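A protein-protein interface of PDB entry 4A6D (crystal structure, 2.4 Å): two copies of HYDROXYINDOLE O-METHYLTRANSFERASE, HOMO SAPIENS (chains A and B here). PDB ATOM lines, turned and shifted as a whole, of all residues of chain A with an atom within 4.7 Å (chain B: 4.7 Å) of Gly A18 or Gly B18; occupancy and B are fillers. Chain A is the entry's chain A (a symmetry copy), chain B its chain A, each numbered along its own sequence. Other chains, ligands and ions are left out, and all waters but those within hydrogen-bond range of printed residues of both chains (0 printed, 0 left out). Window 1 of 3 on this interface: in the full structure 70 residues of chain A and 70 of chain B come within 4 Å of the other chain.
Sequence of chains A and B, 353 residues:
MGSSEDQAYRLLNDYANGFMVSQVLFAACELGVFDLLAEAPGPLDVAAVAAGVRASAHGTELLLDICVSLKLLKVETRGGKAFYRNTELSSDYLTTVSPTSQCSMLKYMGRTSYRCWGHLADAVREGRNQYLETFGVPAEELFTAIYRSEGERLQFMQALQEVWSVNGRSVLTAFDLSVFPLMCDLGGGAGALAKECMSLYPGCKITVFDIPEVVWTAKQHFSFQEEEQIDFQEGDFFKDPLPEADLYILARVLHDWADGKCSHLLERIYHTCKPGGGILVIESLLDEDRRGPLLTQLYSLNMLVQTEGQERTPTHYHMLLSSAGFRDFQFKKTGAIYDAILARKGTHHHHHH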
ATOM      1  N   ASP A  14      -2.827  -7.305 -25.871  1.00  0.00           N
ATOM      2  CA  ASP A  14      -2.291  -8.021 -27.028  1.00  0.00           C
ATOM      3  C   ASP A  14      -1.146  -8.916 -26.583  1.00  0.00           C
ATOM      4  O   ASP A  14      -1.069 -10.091 -26.992  1.00  0.00           O
ATOM      5  CB  ASP A  14      -1.737  -7.010 -28.053  1.00  0.00           C
ATOM      6  CG  ASP A  14      -2.733  -6.360 -28.992  1.00  0.00           C
ATOM      7  OD1 ASP A  14      -3.956  -6.529 -28.776  1.00  0.00           O
ATOM      8  OD2 ASP A  14      -2.286  -5.663 -29.948  1.00  0.00           O
ATOM      9  N   TYR A  15      -0.235  -8.338 -25.761  1.00  0.00           N
ATOM     10  CA  TYR A  15       0.948  -9.029 -25.268  1.00  0.00           C
ATOM     11  C   TYR A  15       0.542 -10.096 -24.288  1.00  0.00           C
ATOM     12  O   TYR A  15       1.035 -11.218 -24.360  1.00  0.00           O
ATOM     13  CB  TYR A  15       1.929  -8.041 -24.597  1.00  0.00           C
ATOM     14  CG  TYR A  15       2.580  -6.986 -25.490  1.00  0.00           C
ATOM     15  CD1 TYR A  15       2.618  -7.138 -26.873  1.00  0.00           C
ATOM     16  CD2 TYR A  15       3.198  -5.868 -24.941  1.00  0.00           C
ATOM     17  CE1 TYR A  15       3.241  -6.202 -27.685  1.00  0.00           C
ATOM     18  CE2 TYR A  15       3.801  -4.909 -25.746  1.00  0.00           C
ATOM     19  CZ  TYR A  15       3.845  -5.092 -27.118  1.00  0.00           C
ATOM     20  OH  TYR A  15       4.427  -4.147 -27.929  1.00  0.00           O
ATOM     21  N   ALA A  16      -0.380  -9.763 -23.369  1.00  0.00           N
ATOM     22  CA  ALA A  16      -0.801 -10.732 -22.370  1.00  0.00           C
ATOM     23  C   ALA A  16      -1.512 -11.936 -22.993  1.00  0.00           C
ATOM     24  O   ALA A  16      -1.345 -13.042 -22.528  1.00  0.00           O
ATOM     25  CB  ALA A  16      -1.686 -10.057 -21.338  1.00  0.00           C
ATOM     26  N   ASN A  17      -2.272 -11.719 -24.061  1.00  0.00           N
ATOM     27  CA  ASN A  17      -3.061 -12.742 -24.734  1.00  0.00           C
ATOM     28  C   ASN A  17      -2.334 -13.535 -25.778  1.00  0.00           C
ATOM     29  O   ASN A  17      -2.898 -14.509 -26.266  1.00  0.00           O
ATOM     30  CB  ASN A  17      -4.282 -12.083 -25.368  1.00  0.00           C
ATOM     31  CG  ASN A  17      -5.256 -11.513 -24.356  1.00  0.00           C
ATOM     32  OD1 ASN A  17      -5.221 -11.822 -23.160  1.00  0.00           O
ATOM     33  ND2 ASN A  17      -6.144 -10.673 -24.820  1.00  0.00           N
ATOM     34  N   GLY A  18      -1.098 -13.136 -26.096  1.00  0.00           N
ATOM     35  CA  GLY A  18      -0.258 -13.735 -27.133  1.00  0.00           C
ATOM     36  C   GLY A  18      -0.108 -15.234 -27.026  1.00  0.00           C
ATOM     37  O   GLY A  18      -0.182 -15.944 -28.034  1.00  0.00           O
ATOM     38  N   PHE A  19       0.051 -15.736 -25.790  1.00  0.00           N
ATOM     39  CA  PHE A  19       0.168 -17.160 -25.548  1.00  0.00           C
ATOM     40  C   PHE A  19      -1.072 -17.951 -26.033  1.00  0.00           C
ATOM     41  O   PHE A  19      -0.909 -19.060 -26.548  1.00  0.00           O
ATOM     42  CB  PHE A  19       0.525 -17.422 -24.090  1.00  0.00           C
ATOM     43  CG  PHE A  19      -0.625 -17.328 -23.115  1.00  0.00           C
ATOM     44  CD1 PHE A  19      -1.421 -18.436 -22.846  1.00  0.00           C
ATOM     45  CD2 PHE A  19      -0.886 -16.144 -22.435  1.00  0.00           C
ATOM     46  CE1 PHE A  19      -2.489 -18.343 -21.961  1.00  0.00           C
ATOM     47  CE2 PHE A  19      -1.946 -16.060 -21.544  1.00  0.00           C
ATOM     48  CZ  PHE A  19      -2.740 -17.159 -21.307  1.00  0.00           C
ATOM     49  N   MET A  20      -2.285 -17.353 -25.928  1.00  0.00           N
ATOM     50  CA  MET A  20      -3.550 -17.950 -26.375  1.00  0.00           C
ATOM     51  C   MET A  20      -3.609 -18.083 -27.899  1.00  0.00           C
ATOM     52  O   MET A  20      -4.046 -19.114 -28.420  1.00  0.00           O
ATOM     53  CB  MET A  20      -4.734 -17.128 -25.876  1.00  0.00           C
ATOM     54  CG  MET A  20      -4.773 -17.023 -24.374  1.00  0.00           C
ATOM     55  SD  MET A  20      -6.353 -16.494 -23.705  1.00  0.00           S
ATOM     56  CE  MET A  20      -6.026 -14.809 -23.465  1.00  0.00           C
ATOM     57  N   VAL A  21      -3.140 -17.034 -28.608  1.00  0.00           N
ATOM     58  CA  VAL A  21      -3.088 -16.972 -30.061  1.00  0.00           C
ATOM     59  C   VAL A  21      -2.068 -18.003 -30.586  1.00  0.00           C
ATOM     60  O   VAL A  21      -2.355 -18.660 -31.589  1.00  0.00           O
ATOM     61  CB  VAL A  21      -2.789 -15.533 -30.524  1.00  0.00           C
ATOM     62  CG1 VAL A  21      -2.412 -15.473 -32.012  1.00  0.00           C
ATOM     63  CG2 VAL A  21      -3.949 -14.611 -30.222  1.00  0.00           C
ATOM     64  N   SER A  22      -0.913 -18.180 -29.889  1.00  0.00           N
ATOM     65  CA  SER A  22       0.106 -19.178 -30.261  1.00  0.00           C
ATOM     66  C   SER A  22      -0.490 -20.564 -30.155  1.00  0.00           C
ATOM     67  O   SER A  22      -0.434 -21.312 -31.122  1.00  0.00           O
ATOM     68  CB  SER A  22       1.361 -19.075 -29.386  1.00  0.00           C
ATOM     69  OG  SER A  22       2.010 -17.829 -29.583  1.00  0.00           O
ATOM     70  N   ASP B  14       4.588 -13.863 -36.017  1.00  0.00           N
ATOM     71  CA  ASP B  14       4.035 -13.043 -34.939  1.00  0.00           C
ATOM     72  C   ASP B  14       3.187 -13.914 -34.026  1.00  0.00           C
ATOM     73  O   ASP B  14       3.291 -13.817 -32.787  1.00  0.00           O
ATOM     74  CB  ASP B  14       3.127 -11.949 -35.535  1.00  0.00           C
ATOM     75  CG  ASP B  14       3.802 -10.698 -36.059  1.00  0.00           C
ATOM     76  OD1 ASP B  14       5.052 -10.689 -36.151  1.00  0.00           O
ATOM     77  OD2 ASP B  14       3.073  -9.720 -36.391  1.00  0.00           O
ATOM     78  N   TYR B  15       2.319 -14.749 -34.651  1.00  0.00           N
ATOM     79  CA  TYR B  15       1.399 -15.624 -33.938  1.00  0.00           C
ATOM     80  C   TYR B  15       2.170 -16.721 -33.254  1.00  0.00           C
ATOM     81  O   TYR B  15       1.915 -17.018 -32.090  1.00  0.00           O
ATOM     82  CB  TYR B  15       0.355 -16.234 -34.901  1.00  0.00           C
ATOM     83  CG  TYR B  15      -0.635 -15.274 -35.558  1.00  0.00           C
ATOM     84  CD1 TYR B  15      -0.862 -14.004 -35.036  1.00  0.00           C
ATOM     85  CD2 TYR B  15      -1.377 -15.661 -36.668  1.00  0.00           C
ATOM     86  CE1 TYR B  15      -1.787 -13.142 -35.606  1.00  0.00           C
ATOM     87  CE2 TYR B  15      -2.286 -14.797 -37.267  1.00  0.00           C
ATOM     88  CZ  TYR B  15      -2.509 -13.546 -36.716  1.00  0.00           C
ATOM     89  OH  TYR B  15      -3.398 -12.675 -37.302  1.00  0.00           O
ATOM     90  N   ALA B  16       3.137 -17.324 -33.964  1.00  0.00           N
ATOM     91  CA  ALA B  16       3.904 -18.413 -33.380  1.00  0.00           C
ATOM     92  C   ALA B  16       4.741 -17.955 -32.183  1.00  0.00           C
ATOM     93  O   ALA B  16       4.883 -18.691 -31.231  1.00  0.00           O
ATOM     94  CB  ALA B  16       4.782 -19.050 -34.441  1.00  0.00           C
ATOM     95  N   ASN B  17       5.258 -16.732 -32.223  1.00  0.00           N
ATOM     96  CA  ASN B  17       6.124 -16.169 -31.196  1.00  0.00           C
ATOM     97  C   ASN B  17       5.421 -15.514 -30.046  1.00  0.00           C
ATOM     98  O   ASN B  17       6.089 -15.161 -29.080  1.00  0.00           O
ATOM     99  CB  ASN B  17       7.065 -15.159 -31.846  1.00  0.00           C
ATOM    100  CG  ASN B  17       8.048 -15.784 -32.816  1.00  0.00           C
ATOM    101  OD1 ASN B  17       8.270 -17.000 -32.839  1.00  0.00           O
ATOM    102  ND2 ASN B  17       8.656 -14.962 -33.630  1.00  0.00           N
ATOM    103  N   GLY B  18       4.095 -15.376 -30.142  1.00  0.00           N
ATOM    104  CA  GLY B  18       3.243 -14.705 -29.160  1.00  0.00           C
ATOM    105  C   GLY B  18       3.426 -15.190 -27.740  1.00  0.00           C
ATOM    106  O   GLY B  18       3.484 -14.383 -26.807  1.00  0.00           O
ATOM    107  N   PHE B  19       3.574 -16.514 -27.571  1.00  0.00           N
ATOM    108  CA  PHE B  19       3.796 -17.101 -26.265  1.00  0.00           C
ATOM    109  C   PHE B  19       5.079 -16.569 -25.581  1.00  0.00           C
ATOM    110  O   PHE B  19       5.069 -16.373 -24.364  1.00  0.00           O
ATOM    111  CB  PHE B  19       3.739 -18.622 -26.352  1.00  0.00           C
ATOM    112  CG  PHE B  19       4.985 -19.286 -26.887  1.00  0.00           C
ATOM    113  CD1 PHE B  19       6.026 -19.636 -26.035  1.00  0.00           C
ATOM    114  CD2 PHE B  19       5.099 -19.601 -28.236  1.00  0.00           C
ATOM    115  CE1 PHE B  19       7.178 -20.234 -26.532  1.00  0.00           C
ATOM    116  CE2 PHE B  19       6.247 -20.208 -28.726  1.00  0.00           C
ATOM    117  CZ  PHE B  19       7.279 -20.525 -27.872  1.00  0.00           C
ATOM    118  N   MET B  20       6.142 -16.277 -26.372  1.00  0.00           N
ATOM    119  CA  MET B  20       7.416 -15.729 -25.886  1.00  0.00           C
ATOM    120  C   MET B  20       7.256 -14.300 -25.359  1.00  0.00           C
ATOM    121  O   MET B  20       7.809 -13.956 -24.310  1.00  0.00           O
ATOM    122  CB  MET B  20       8.468 -15.764 -26.990  1.00  0.00           C
ATOM    123  CG  MET B  20       8.723 -17.159 -27.500  1.00  0.00           C
ATOM    124  SD  MET B  20      10.245 -17.341 -28.436  1.00  0.00           S
ATOM    125  CE  MET B  20       9.618 -17.243 -30.048  1.00  0.00           C
ATOM    126  N   VAL B  21       6.473 -13.478 -26.090  1.00  0.00           N
ATOM    127  CA  VAL B  21       6.178 -12.095 -25.749  1.00  0.00           C
ATOM    128  C   VAL B  21       5.323 -12.050 -24.465  1.00  0.00           C
ATOM    129  O   VAL B  21       5.577 -11.192 -23.617  1.00  0.00           O
ATOM    130  CB  VAL B  21       5.516 -11.380 -26.943  1.00  0.00           C
ATOM    131  CG1 VAL B  21       4.903 -10.031 -26.539  1.00  0.00           C
ATOM    132  CG2 VAL B  21       6.492 -11.210 -28.086  1.00  0.00           C
ATOM    133  N   SER B  22       4.357 -12.993 -24.300  1.00  0.00           N
ATOM    134  CA  SER B  22       3.521 -13.086 -23.090  1.00  0.00           C
ATOM    135  C   SER B  22       4.401 -13.387 -21.897  1.00  0.00           C
ATOM    136  O   SER B  22       4.348 -12.655 -20.917  1.00  0.00           O
ATOM    137  CB  SER B  22       2.429 -14.153 -23.222  1.00  0.00           C
ATOM    138  OG  SER B  22       1.512 -13.809 -24.249  1.00  0.00           O
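OG of Ser A22 is in hydrogen-bond range of O of Tyr B15, 2.6 Å away. O of Ala B16 sits at hydrogen-bond distance from OG of Ser A22 (3.4 Å). The side-chain hydroxyl of Ser A22 is in hydrogen-bond range of the backbone NH of Gly B18. N of Phe B19 sits at hydrogen-bond distance from OG of Ser A22 (2.9 Å). OG of Ser B22 lies within hydrogen-bond range of O of Tyr A15, at 2.6 Å. The side-chain hydroxyl (OG) of Ser B22 lies within hydrogen-bond range of the backbone carbonyl oxygen (O) of Ala A16, 3.4 Å away. The backbone NH of Gly A18 is in hydrogen-bond range of the side-chain hydroxyl of Ser B22, 3.3 Å away. The backbone NH of Phe A19 sits at hydrogen-bond distance from the side-chain hydroxyl of Ser B22, 2.9 Å away.
OG of Ser B22 lies within hydrogen-bond range of O of Gly B18, 3.3 Å away. The side-chain hydroxyl (OG) of Ser A22 is in hydrogen-bond range of the backbone carbonyl oxygen (O) of Gly A18, at 3.3 Å.
Among the printed residues, pairs that only touch across the chains: Gly A18 with Gly B18 (3.6 Å), Phe A19 with Phe B19 (3.7 Å), Tyr A15 with Val B21 (3.7 Å), Val A21 with Tyr B15 (3.7 Å), Gly A18 with Phe B19 (3.8 Å) and Phe A19 with Gly B18 (3.8 Å).
Printed residues of chain B within 4 Å of Gly A18: Gly B18, Phe B19 and Ser B22. Gly B18 touches just these residues of chain A: Gly A18 (3.6 Å), Phe A19 (3.8 Å) and Ser A22 (3.3 Å). Of the printed residues of chain A, Tyr B15 touches Val A21 (3.7 Å) and Ser A22 (2.6 Å). Printed residues of chain A within 4 Å of Ala B16: Ser A22 (3.4 Å). Printed residues of chain B within 4 Å of Ala A16: Ser B22 (3.4 Å). Printed residues of chain B within 4 Å of Tyr A15: Val B21 (3.7 Å) and Ser B22 (2.6 Å). The nearest printed residue of chain A that does not touch Gly B18 is Tyr A15 (4.7 Å). The nearest printed residue of chain B that does not touch Phe A19 is Met B20 (6.1 Å).
Printed residues of chain B that touch a printed residue of chain A: Tyr B15, Ala B16, Gly B18, Phe B19, Val B21 and Ser B22. Hydrophobic or aromatic side chains of chain B that line the printed part of chain A: Tyr B15, Phe B19 and Val B21. Along chain B the printed residues that touch a printed residue of chain A span positions 15 to 22. Hydrophobic or aromatic side chains of chain A within 4 Å of the printed part of chain B: Tyr A15, Phe A19 and Val A21.
Tyr A15 touches Val B21, and with the chains exchanged Val A21 touches Tyr B15. Gly A18 touches Phe B19, and with the chains exchanged Phe A19 touches Gly B18. Phe A19 touches its own counterpart, Phe B19. Phe A19 touches Ser B22, and with the chains exchanged Ser A22 touches Phe B19. Of the 14 pairs that touch across the chains among the printed residues, 14 have their exchanged pair printed and touching as well.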
